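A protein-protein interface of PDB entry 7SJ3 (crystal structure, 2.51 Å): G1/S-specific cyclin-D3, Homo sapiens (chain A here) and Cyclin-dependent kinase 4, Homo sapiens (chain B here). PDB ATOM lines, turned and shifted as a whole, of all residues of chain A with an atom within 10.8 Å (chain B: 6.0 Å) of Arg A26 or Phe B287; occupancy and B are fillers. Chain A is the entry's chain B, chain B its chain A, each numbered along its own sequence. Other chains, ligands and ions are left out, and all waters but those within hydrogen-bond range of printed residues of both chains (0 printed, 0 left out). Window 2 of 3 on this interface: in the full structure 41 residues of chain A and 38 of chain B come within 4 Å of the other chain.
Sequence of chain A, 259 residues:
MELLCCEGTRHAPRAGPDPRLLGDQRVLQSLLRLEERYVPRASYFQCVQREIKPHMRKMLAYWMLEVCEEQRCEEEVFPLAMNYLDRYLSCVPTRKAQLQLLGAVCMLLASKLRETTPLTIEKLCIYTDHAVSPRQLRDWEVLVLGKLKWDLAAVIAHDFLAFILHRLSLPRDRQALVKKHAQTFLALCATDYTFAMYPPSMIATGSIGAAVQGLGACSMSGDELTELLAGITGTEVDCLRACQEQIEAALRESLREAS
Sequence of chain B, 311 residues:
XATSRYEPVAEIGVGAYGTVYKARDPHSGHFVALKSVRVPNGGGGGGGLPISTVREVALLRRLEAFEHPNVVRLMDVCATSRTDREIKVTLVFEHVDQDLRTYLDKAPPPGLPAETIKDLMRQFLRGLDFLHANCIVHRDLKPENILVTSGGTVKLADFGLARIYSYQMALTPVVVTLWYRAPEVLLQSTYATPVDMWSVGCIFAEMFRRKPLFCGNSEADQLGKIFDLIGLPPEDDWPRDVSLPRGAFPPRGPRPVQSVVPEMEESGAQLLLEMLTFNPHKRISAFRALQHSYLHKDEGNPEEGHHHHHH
OD2 of Asp B129 is in salt-bridge range of NH1 of Arg A26 (2.9 Å).
OD2 of Asp A24 lies within salt-bridge range of NH2 of Arg A26 (2.8 Å).
The backbone carbonyl oxygen of Phe B287 lies close to the side-chain amide oxygen of Gln B291.
The backbone NH of Arg B288 lies close to the side-chain hydroxyl of Ser B285, at 3.1 Å.
N of Ser B285 touches NH2 of Arg A20, 3.7 Å away.
Phe B287 touches Arg A26.
Val A27 touches Ala B133 (CA to O, 3.6 Å).
Ala B133 touches Ser A30.
Arg A26 touches just these residues of chain B: Asp B129 and Phe B287.
Phe B287 touches just one residue of chain A: Arg A26 (3.5 Å).
Asp B129 touches just one residue of chain A: Arg A26.
Ser B285 touches just one residue of chain A: Arg A20.
No residue of chain A comes within 4 Å of Ala B286.
No residue of chain A comes within 4 Å of Ala B289.
No residue of chain A comes within 4 Å of Leu B290.
No residue of chain A comes within 4 Å of Gln B291.
Printed residues of chain B within 4 Å of Val A27: Ala B133.
Of the printed residues of chain B, Arg A20 touches Ser B285 (3.7 Å).
Of the printed residues of chain B, Ser A30 touches Ala B133.
The nearest residue of chain B that does not touch Arg A26 is Ala B133 (4.1 Å).
The nearest residue of chain A that does not touch Phe B287 is Asp A24 (6.0 Å).
Hydrophobic or aromatic side chains of chain B within 4 Å of the printed part of chain A: Phe B287.
Hydrophobic or aromatic side chains of chain A that line the printed part of chain B: Val A27.
Among the printed residues, Asp or Glu carboxylates within 4 Å of a Lys or Arg side-chain nitrogen of the other chain: Arg A26 with Asp B129 (2.9 Å).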
ATOM      1  N   PRO A  19      13.139 -28.500  -1.999  1.00  0.00           N
ATOM      2  CA  PRO A  19      13.230 -28.549  -0.531  1.00  0.00           C
ATOM      3  C   PRO A  19      12.429 -27.462   0.156  1.00  0.00           C
ATOM      4  O   PRO A  19      12.064 -27.630   1.328  1.00  0.00           O
ATOM      5  CB  PRO A  19      14.731 -28.375  -0.265  1.00  0.00           C
ATOM      6  CG  PRO A  19      15.232 -27.620  -1.455  1.00  0.00           C
ATOM      7  CD  PRO A  19      14.407 -28.076  -2.621  1.00  0.00           C
ATOM      8  N   ARG A  20      12.143 -26.357  -0.537  1.00  0.00           N
ATOM      9  CA  ARG A  20      11.290 -25.315   0.024  1.00  0.00           C
ATOM     10  C   ARG A  20       9.870 -25.818   0.258  1.00  0.00           C
ATOM     11  O   ARG A  20       9.170 -25.307   1.140  1.00  0.00           O
ATOM     12  CB  ARG A  20      11.298 -24.080  -0.883  1.00  0.00           C
ATOM     13  CG  ARG A  20      12.704 -23.610  -1.272  1.00  0.00           C
ATOM     14  CD  ARG A  20      12.712 -22.188  -1.834  1.00  0.00           C
ATOM     15  NE  ARG A  20      13.168 -21.203  -0.855  1.00  0.00           N
ATOM     16  CZ  ARG A  20      14.443 -20.986  -0.543  1.00  0.00           C
ATOM     17  NH1 ARG A  20      15.401 -21.688  -1.132  1.00  0.00           N
ATOM     18  NH2 ARG A  20      14.763 -20.068   0.362  1.00  0.00           N
ATOM     19  N   LEU A  21       9.426 -26.807  -0.518  1.00  0.00           N
ATOM     20  CA  LEU A  21       8.103 -27.398  -0.352  1.00  0.00           C
ATOM     21  C   LEU A  21       8.119 -28.624   0.559  1.00  0.00           C
ATOM     22  O   LEU A  21       7.331 -28.701   1.507  1.00  0.00           O
ATOM     23  CB  LEU A  21       7.525 -27.775  -1.722  1.00  0.00           C
ATOM     24  CG  LEU A  21       7.215 -26.679  -2.739  1.00  0.00           C
ATOM     25  CD1 LEU A  21       6.485 -27.256  -3.939  1.00  0.00           C
ATOM     26  CD2 LEU A  21       6.357 -25.604  -2.087  1.00  0.00           C
ATOM     27  N   LEU A  22       9.019 -29.576   0.301  1.00  0.00           N
ATOM     28  CA  LEU A  22       9.019 -30.822   1.062  1.00  0.00           C
ATOM     29  C   LEU A  22       9.355 -30.590   2.530  1.00  0.00           C
ATOM     30  O   LEU A  22       8.907 -31.354   3.393  1.00  0.00           O
ATOM     31  CB  LEU A  22       9.991 -31.821   0.433  1.00  0.00           C
ATOM     32  CG  LEU A  22       9.679 -32.180  -1.024  1.00  0.00           C
ATOM     33  CD1 LEU A  22      10.743 -33.096  -1.597  1.00  0.00           C
ATOM     34  CD2 LEU A  22       8.282 -32.784  -1.171  1.00  0.00           C
ATOM     35  N   GLY A  23      10.204 -29.605   2.823  1.00  0.00           N
ATOM     36  CA  GLY A  23      10.637 -29.319   4.177  1.00  0.00           C
ATOM     37  C   GLY A  23       9.803 -28.315   4.945  1.00  0.00           C
ATOM     38  O   GLY A  23       9.995 -28.166   6.155  1.00  0.00           O
ATOM     39  N   ASP A  24       8.876 -27.620   4.286  1.00  0.00           N
ATOM     40  CA  ASP A  24       8.028 -26.635   4.954  1.00  0.00           C
ATOM     41  C   ASP A  24       6.811 -27.368   5.504  1.00  0.00           C
ATOM     42  O   ASP A  24       5.959 -27.835   4.739  1.00  0.00           O
ATOM     43  CB  ASP A  24       7.612 -25.524   3.991  1.00  0.00           C
ATOM     44  CG  ASP A  24       6.750 -24.453   4.655  1.00  0.00           C
ATOM     45  OD1 ASP A  24       6.523 -24.524   5.881  1.00  0.00           O
ATOM     46  OD2 ASP A  24       6.279 -23.544   3.938  1.00  0.00           O
ATOM     47  N   GLN A  25       6.742 -27.482   6.833  1.00  0.00           N
ATOM     48  CA  GLN A  25       5.663 -28.236   7.460  1.00  0.00           C
ATOM     49  C   GLN A  25       4.286 -27.687   7.102  1.00  0.00           C
ATOM     50  O   GLN A  25       3.310 -28.445   7.074  1.00  0.00           O
ATOM     51  CB  GLN A  25       5.864 -28.252   8.975  1.00  0.00           C
ATOM     52  CG  GLN A  25       4.809 -29.029   9.733  1.00  0.00           C
ATOM     53  CD  GLN A  25       4.712 -30.471   9.256  1.00  0.00           C
ATOM     54  OE1 GLN A  25       5.725 -31.117   8.987  1.00  0.00           O
ATOM     55  NE2 GLN A  25       3.493 -30.990   9.179  1.00  0.00           N
ATOM     56  N   ARG A  26       4.182 -26.385   6.814  1.00  0.00           N
ATOM     57  CA  ARG A  26       2.870 -25.824   6.511  1.00  0.00           C
ATOM     58  C   ARG A  26       2.306 -26.415   5.228  1.00  0.00           C
ATOM     59  O   ARG A  26       1.086 -26.543   5.091  1.00  0.00           O
ATOM     60  CB  ARG A  26       2.927 -24.303   6.374  1.00  0.00           C
ATOM     61  CG  ARG A  26       3.405 -23.533   7.587  1.00  0.00           C
ATOM     62  CD  ARG A  26       3.561 -22.076   7.197  1.00  0.00           C
ATOM     63  NE  ARG A  26       4.474 -21.939   6.066  1.00  0.00           N
ATOM     64  CZ  ARG A  26       4.490 -20.903   5.233  1.00  0.00           C
ATOM     65  NH1 ARG A  26       3.634 -19.901   5.393  1.00  0.00           N
ATOM     66  NH2 ARG A  26       5.353 -20.877   4.226  1.00  0.00           N
ATOM     67  N   VAL A  27       3.176 -26.813   4.297  1.00  0.00           N
ATOM     68  CA  VAL A  27       2.702 -27.375   3.037  1.00  0.00           C
ATOM     69  C   VAL A  27       2.003 -28.703   3.290  1.00  0.00           C
ATOM     70  O   VAL A  27       0.905 -28.953   2.780  1.00  0.00           O
ATOM     71  CB  VAL A  27       3.868 -27.542   2.046  1.00  0.00           C
ATOM     72  CG1 VAL A  27       3.358 -28.082   0.727  1.00  0.00           C
ATOM     73  CG2 VAL A  27       4.586 -26.226   1.825  1.00  0.00           C
ATOM     74  N   LEU A  28       2.633 -29.574   4.080  1.00  0.00           N
ATOM     75  CA  LEU A  28       2.001 -30.837   4.442  1.00  0.00           C
ATOM     76  C   LEU A  28       0.722 -30.597   5.238  1.00  0.00           C
ATOM     77  O   LEU A  28      -0.293 -31.271   5.023  1.00  0.00           O
ATOM     78  CB  LEU A  28       2.976 -31.705   5.238  1.00  0.00           C
ATOM     79  CG  LEU A  28       2.429 -33.060   5.696  1.00  0.00           C
ATOM     80  CD1 LEU A  28       1.981 -33.877   4.500  1.00  0.00           C
ATOM     81  CD2 LEU A  28       3.457 -33.822   6.526  1.00  0.00           C
ATOM     82  N   GLN A  29       0.761 -29.647   6.177  1.00  0.00           N
ATOM     83  CA  GLN A  29      -0.437 -29.314   6.941  1.00  0.00           C
ATOM     84  C   GLN A  29      -1.559 -28.816   6.034  1.00  0.00           C
ATOM     85  O   GLN A  29      -2.738 -29.087   6.290  1.00  0.00           O
ATOM     86  CB  GLN A  29      -0.102 -28.267   8.003  1.00  0.00           C
ATOM     87  CG  GLN A  29      -0.951 -28.380   9.256  1.00  0.00           C
ATOM     88  CD  GLN A  29      -0.707 -29.680  10.002  1.00  0.00           C
ATOM     89  OE1 GLN A  29       0.436 -30.045  10.283  1.00  0.00           O
ATOM     90  NE2 GLN A  29      -1.783 -30.389  10.324  1.00  0.00           N
ATOM     91  N   SER A  30      -1.214 -28.069   4.982  1.00  0.00           N
ATOM     92  CA  SER A  30      -2.225 -27.592   4.042  1.00  0.00           C
ATOM     93  C   SER A  30      -2.897 -28.750   3.310  1.00  0.00           C
ATOM     94  O   SER A  30      -4.124 -28.768   3.156  1.00  0.00           O
ATOM     95  CB  SER A  30      -1.600 -26.614   3.050  1.00  0.00           C
ATOM     96  OG  SER A  30      -2.469 -26.362   1.960  1.00  0.00           O
ATOM     97  N   LEU A  31      -2.106 -29.723   2.845  1.00  0.00           N
ATOM     98  CA  LEU A  31      -2.670 -30.893   2.177  1.00  0.00           C
ATOM     99  C   LEU A  31      -3.565 -31.689   3.117  1.00  0.00           C
ATOM    100  O   LEU A  31      -4.662 -32.113   2.733  1.00  0.00           O
ATOM    101  CB  LEU A  31      -1.550 -31.785   1.630  1.00  0.00           C
ATOM    102  CG  LEU A  31      -0.548 -31.148   0.663  1.00  0.00           C
ATOM    103  CD1 LEU A  31       0.423 -32.183   0.100  1.00  0.00           C
ATOM    104  CD2 LEU A  31      -1.294 -30.469  -0.464  1.00  0.00           C
ATOM    105  N   LEU A  32      -3.128 -31.871   4.364  1.00  0.00           N
ATOM    106  CA  LEU A  32      -3.923 -32.627   5.326  1.00  0.00           C
ATOM    107  C   LEU A  32      -5.253 -31.937   5.571  1.00  0.00           C
ATOM    108  O   LEU A  32      -6.275 -32.598   5.793  1.00  0.00           O
ATOM    109  CB  LEU A  32      -3.147 -32.825   6.628  1.00  0.00           C
ATOM    110  CG  LEU A  32      -1.877 -33.671   6.510  1.00  0.00           C
ATOM    111  CD1 LEU A  32      -1.093 -33.625   7.806  1.00  0.00           C
ATOM    112  CD2 LEU A  32      -2.210 -35.105   6.133  1.00  0.00           C
ATOM    113  N   ARG A  33      -5.252 -30.603   5.563  1.00  0.00           N
ATOM    114  CA  ARG A  33      -6.493 -29.867   5.756  1.00  0.00           C
ATOM    115  C   ARG A  33      -7.382 -29.944   4.522  1.00  0.00           C
ATOM    116  O   ARG A  33      -8.610 -29.993   4.650  1.00  0.00           O
ATOM    117  CB  ARG A  33      -6.184 -28.407   6.081  1.00  0.00           C
ATOM    118  CG  ARG A  33      -6.765 -27.918   7.388  1.00  0.00           C
ATOM    119  CD  ARG A  33      -6.503 -26.427   7.598  1.00  0.00           C
ATOM    120  NE  ARG A  33      -5.091 -26.126   7.831  1.00  0.00           N
ATOM    121  CZ  ARG A  33      -4.286 -25.552   6.942  1.00  0.00           C
ATOM    122  NH1 ARG A  33      -4.752 -25.208   5.748  1.00  0.00           N
ATOM    123  NH2 ARG A  33      -3.016 -25.315   7.247  1.00  0.00           N
ATOM    124  N   LEU A  34      -6.790 -30.035   3.328  1.00  0.00           N
ATOM    125  CA  LEU A  34      -7.582 -30.034   2.104  1.00  0.00           C
ATOM    126  C   LEU A  34      -8.176 -31.397   1.774  1.00  0.00           C
ATOM    127  O   LEU A  34      -9.198 -31.462   1.087  1.00  0.00           O
ATOM    128  CB  LEU A  34      -6.728 -29.586   0.917  1.00  0.00           C
ATOM    129  CG  LEU A  34      -6.593 -28.104   0.598  1.00  0.00           C
ATOM    130  CD1 LEU A  34      -5.541 -27.919  -0.479  1.00  0.00           C
ATOM    131  CD2 LEU A  34      -7.934 -27.537   0.152  1.00  0.00           C
ATOM    132  N   PHE A 160       1.022 -37.216  -1.422  1.00  0.00           N
ATOM    133  CA  PHE A 160       1.703 -37.287  -0.134  1.00  0.00           C
ATOM    134  C   PHE A 160       3.009 -38.062  -0.205  1.00  0.00           C
ATOM    135  O   PHE A 160       3.831 -37.954   0.715  1.00  0.00           O
ATOM    136  CB  PHE A 160       0.790 -37.939   0.918  1.00  0.00           C
ATOM    137  CG  PHE A 160      -0.372 -37.072   1.357  1.00  0.00           C
ATOM    138  CD1 PHE A 160      -0.218 -36.141   2.368  1.00  0.00           C
ATOM    139  CD2 PHE A 160      -1.610 -37.200   0.763  1.00  0.00           C
ATOM    140  CE1 PHE A 160      -1.273 -35.352   2.777  1.00  0.00           C
ATOM    141  CE2 PHE A 160      -2.670 -36.419   1.168  1.00  0.00           C
ATOM    142  CZ  PHE A 160      -2.503 -35.492   2.175  1.00  0.00           C
ATOM    143  N   PHE A 163       6.280 -36.178   0.242  1.00  0.00           N
ATOM    144  CA  PHE A 163       6.381 -35.552   1.561  1.00  0.00           C
ATOM    145  C   PHE A 163       6.739 -36.572   2.632  1.00  0.00           C
ATOM    146  O   PHE A 163       7.555 -36.291   3.518  1.00  0.00           O
ATOM    147  CB  PHE A 163       5.079 -34.825   1.914  1.00  0.00           C
ATOM    148  CG  PHE A 163       4.821 -33.613   1.063  1.00  0.00           C
ATOM    149  CD1 PHE A 163       5.343 -32.389   1.432  1.00  0.00           C
ATOM    150  CD2 PHE A 163       4.071 -33.694  -0.100  1.00  0.00           C
ATOM    151  CE1 PHE A 163       5.133 -31.262   0.659  1.00  0.00           C
ATOM    152  CE2 PHE A 163       3.851 -32.570  -0.881  1.00  0.00           C
ATOM    153  CZ  PHE A 163       4.380 -31.350  -0.500  1.00  0.00           C
ATOM    154  N   ARG A 167      10.604 -37.481   4.912  1.00  0.00           N
ATOM    155  CA  ARG A 167      10.752 -37.586   6.349  1.00  0.00           C
ATOM    156  C   ARG A 167      11.318 -38.929   6.785  1.00  0.00           C
ATOM    157  O   ARG A 167      11.432 -39.179   7.992  1.00  0.00           O
ATOM    158  CB  ARG A 167       9.408 -37.307   7.018  1.00  0.00           C
ATOM    159  CG  ARG A 167       9.104 -35.814   7.080  1.00  0.00           C
ATOM    160  CD  ARG A 167       7.635 -35.501   6.906  1.00  0.00           C
ATOM    161  NE  ARG A 167       7.380 -34.062   7.001  1.00  0.00           N
ATOM    162  CZ  ARG A 167       7.426 -33.219   5.970  1.00  0.00           C
ATOM    163  NH1 ARG A 167       7.725 -33.662   4.751  1.00  0.00           N
ATOM    164  NH2 ARG A 167       7.172 -31.926   6.155  1.00  0.00           N
ATOM    165  N   ILE A 232       3.566 -38.734  11.225  1.00  0.00           N
ATOM    166  CA  ILE A 232       3.772 -37.780  10.139  1.00  0.00           C
ATOM    167  C   ILE A 232       2.455 -37.127   9.733  1.00  0.00           C
ATOM    168  O   ILE A 232       2.394 -35.916   9.484  1.00  0.00           O
ATOM    169  CB  ILE A 232       4.434 -38.482   8.937  1.00  0.00           C
ATOM    170  CG1 ILE A 232       5.907 -38.783   9.220  1.00  0.00           C
ATOM    171  CG2 ILE A 232       4.278 -37.645   7.682  1.00  0.00           C
ATOM    172  CD1 ILE A 232       6.551 -39.718   8.211  1.00  0.00           C
ATOM    173  N   LEU B 125       3.563 -10.322  -0.825  1.00  0.00           N
ATOM    174  CA  LEU B 125       4.285 -11.485  -0.319  1.00  0.00           C
ATOM    175  C   LEU B 125       3.353 -12.453   0.402  1.00  0.00           C
ATOM    176  O   LEU B 125       3.502 -13.673   0.274  1.00  0.00           O
ATOM    177  CB  LEU B 125       5.412 -11.038   0.611  1.00  0.00           C
ATOM    178  CG  LEU B 125       6.620 -10.349  -0.026  1.00  0.00           C
ATOM    179  CD1 LEU B 125       7.538  -9.791   1.050  1.00  0.00           C
ATOM    180  CD2 LEU B 125       7.373 -11.320  -0.917  1.00  0.00           C
ATOM    181  N   ASP B 129       3.118 -16.241  -0.680  1.00  0.00           N
ATOM    182  CA  ASP B 129       3.414 -17.247   0.334  1.00  0.00           C
ATOM    183  C   ASP B 129       2.231 -18.185   0.532  1.00  0.00           C
ATOM    184  O   ASP B 129       2.415 -19.390   0.737  1.00  0.00           O
ATOM    185  CB  ASP B 129       3.787 -16.573   1.653  1.00  0.00           C
ATOM    186  CG  ASP B 129       4.089 -17.568   2.761  1.00  0.00           C
ATOM    187  OD1 ASP B 129       4.988 -18.420   2.584  1.00  0.00           O
ATOM    188  OD2 ASP B 129       3.416 -17.497   3.811  1.00  0.00           O
ATOM    189  N   ALA B 133       2.735 -21.997  -0.097  1.00  0.00           N
ATOM    190  CA  ALA B 133       2.336 -22.881   0.992  1.00  0.00           C
ATOM    191  C   ALA B 133       1.207 -23.822   0.596  1.00  0.00           C
ATOM    192  O   ALA B 133       0.913 -24.763   1.344  1.00  0.00           O
ATOM    193  CB  ALA B 133       1.916 -22.052   2.208  1.00  0.00           C
ATOM    194  N   MET B 197       9.602 -15.813  -7.165  1.00  0.00           N
ATOM    195  CA  MET B 197      10.315 -14.872  -6.316  1.00  0.00           C
ATOM    196  C   MET B 197      11.196 -13.944  -7.139  1.00  0.00           C
ATOM    197  O   MET B 197      11.423 -12.793  -6.745  1.00  0.00           O
ATOM    198  CB  MET B 197      11.136 -15.623  -5.276  1.00  0.00           C
ATOM    199  CG  MET B 197      11.343 -14.803  -4.034  1.00  0.00           C
ATOM    200  SD  MET B 197       9.746 -14.337  -3.334  1.00  0.00           S
ATOM    201  CE  MET B 197      10.251 -13.135  -2.111  1.00  0.00           C
ATOM    202  N   SER B 285      12.923 -16.922   0.121  1.00  0.00           N
ATOM    203  CA  SER B 285      11.547 -17.364  -0.035  1.00  0.00           C
ATOM    204  C   SER B 285      10.592 -16.218   0.277  1.00  0.00           C
ATOM    205  O   SER B 285      10.973 -15.192   0.846  1.00  0.00           O
ATOM    206  CB  SER B 285      11.242 -18.559   0.867  1.00  0.00           C
ATOM    207  OG  SER B 285      11.242 -18.179   2.228  1.00  0.00           O
ATOM    208  N   ALA B 286       9.327 -16.403  -0.109  1.00  0.00           N
ATOM    209  CA  ALA B 286       8.313 -15.402   0.201  1.00  0.00           C
ATOM    210  C   ALA B 286       8.121 -15.270   1.706  1.00  0.00           C
ATOM    211  O   ALA B 286       7.908 -14.165   2.221  1.00  0.00           O
ATOM    212  CB  ALA B 286       6.994 -15.763  -0.478  1.00  0.00           C
ATOM    213  N   PHE B 287       8.224 -16.384   2.431  1.00  0.00           N
ATOM    214  CA  PHE B 287       8.045 -16.351   3.878  1.00  0.00           C
ATOM    215  C   PHE B 287       9.168 -15.574   4.548  1.00  0.00           C
ATOM    216  O   PHE B 287       8.918 -14.703   5.389  1.00  0.00           O
ATOM    217  CB  PHE B 287       7.974 -17.774   4.428  1.00  0.00           C
ATOM    218  CG  PHE B 287       7.691 -17.839   5.901  1.00  0.00           C
ATOM    219  CD1 PHE B 287       8.735 -17.826   6.815  1.00  0.00           C
ATOM    220  CD2 PHE B 287       6.393 -17.910   6.376  1.00  0.00           C
ATOM    221  CE1 PHE B 287       8.491 -17.882   8.171  1.00  0.00           C
ATOM    222  CE2 PHE B 287       6.140 -17.970   7.737  1.00  0.00           C
ATOM    223  CZ  PHE B 287       7.191 -17.955   8.634  1.00  0.00           C
ATOM    224  N   ARG B 288      10.415 -15.864   4.174  1.00  0.00           N
ATOM    225  CA  ARG B 288      11.545 -15.173   4.783  1.00  0.00           C
ATOM    226  C   ARG B 288      11.559 -13.693   4.423  1.00  0.00           C
ATOM    227  O   ARG B 288      12.004 -12.868   5.229  1.00  0.00           O
ATOM    228  CB  ARG B 288      12.862 -15.827   4.356  1.00  0.00           C
ATOM    229  CG  ARG B 288      12.957 -17.319   4.649  1.00  0.00           C
ATOM    230  CD  ARG B 288      12.877 -17.624   6.137  1.00  0.00           C
ATOM    231  NE  ARG B 288      14.023 -17.092   6.867  1.00  0.00           N
ATOM    232  CZ  ARG B 288      13.977 -16.030   7.664  1.00  0.00           C
ATOM    233  NH1 ARG B 288      12.835 -15.384   7.846  1.00  0.00           N
ATOM    234  NH2 ARG B 288      15.074 -15.618   8.286  1.00  0.00           N
ATOM    235  N   ALA B 289      11.089 -13.335   3.226  1.00  0.00           N
ATOM    236  CA  ALA B 289      11.009 -11.921   2.866  1.00  0.00           C
ATOM    237  C   ALA B 289      10.001 -11.180   3.739  1.00  0.00           C
ATOM    238  O   ALA B 289      10.215 -10.012   4.086  1.00  0.00           O
ATOM    239  CB  ALA B 289      10.651 -11.776   1.387  1.00  0.00           C
ATOM    240  N   LEU B 290       8.891 -11.831   4.097  1.00  0.00           N
ATOM    241  CA  LEU B 290       7.921 -11.218   5.000  1.00  0.00           C
ATOM    242  C   LEU B 290       8.485 -11.002   6.401  1.00  0.00           C
ATOM    243  O   LEU B 290       7.949 -10.180   7.153  1.00  0.00           O
ATOM    244  CB  LEU B 290       6.659 -12.072   5.068  1.00  0.00           C
ATOM    245  CG  LEU B 290       5.323 -11.335   5.181  1.00  0.00           C
ATOM    246  CD1 LEU B 290       5.247 -10.166   4.208  1.00  0.00           C
ATOM    247  CD2 LEU B 290       4.184 -12.303   4.943  1.00  0.00           C
ATOM    248  N   GLN B 291       9.542 -11.727   6.762  1.00  0.00           N
ATOM    249  CA  GLN B 291      10.232 -11.625   8.043  1.00  0.00           C
ATOM    250  C   GLN B 291      11.434 -10.694   7.983  1.00  0.00           C
ATOM    251  O   GLN B 291      12.161 -10.567   8.975  1.00  0.00           O
ATOM    252  CB  GLN B 291      10.682 -13.011   8.514  1.00  0.00           C
ATOM    253  CG  GLN B 291       9.741 -13.685   9.498  1.00  0.00           C
ATOM    254  CD  GLN B 291       8.298 -13.645   9.043  1.00  0.00           C
ATOM    255  OE1 GLN B 291       7.940 -14.245   8.029  1.00  0.00           O
ATOM    256  NE2 GLN B 291       7.458 -12.940   9.792  1.00  0.00           N
ATOM    257  N   HIS B 292      11.656 -10.055   6.842  1.00  0.00           N
ATOM    258  CA  HIS B 292      12.772  -9.143   6.652  1.00  0.00           C
ATOM    259  C   HIS B 292      12.609  -7.877   7.488  1.00  0.00           C
ATOM    260  O   HIS B 292      11.497  -7.428   7.781  1.00  0.00           O
ATOM    261  CB  HIS B 292      12.909  -8.782   5.173  1.00  0.00           C
ATOM    262  CG  HIS B 292      14.258  -8.249   4.800  1.00  0.00           C
ATOM    263  ND1 HIS B 292      14.615  -6.932   4.988  1.00  0.00           N
ATOM    264  CD2 HIS B 292      15.335  -8.855   4.249  1.00  0.00           C
ATOM    265  CE1 HIS B 292      15.855  -6.750   4.572  1.00  0.00           C
ATOM    266  NE2 HIS B 292      16.315  -7.901   4.116  1.00  0.00           N
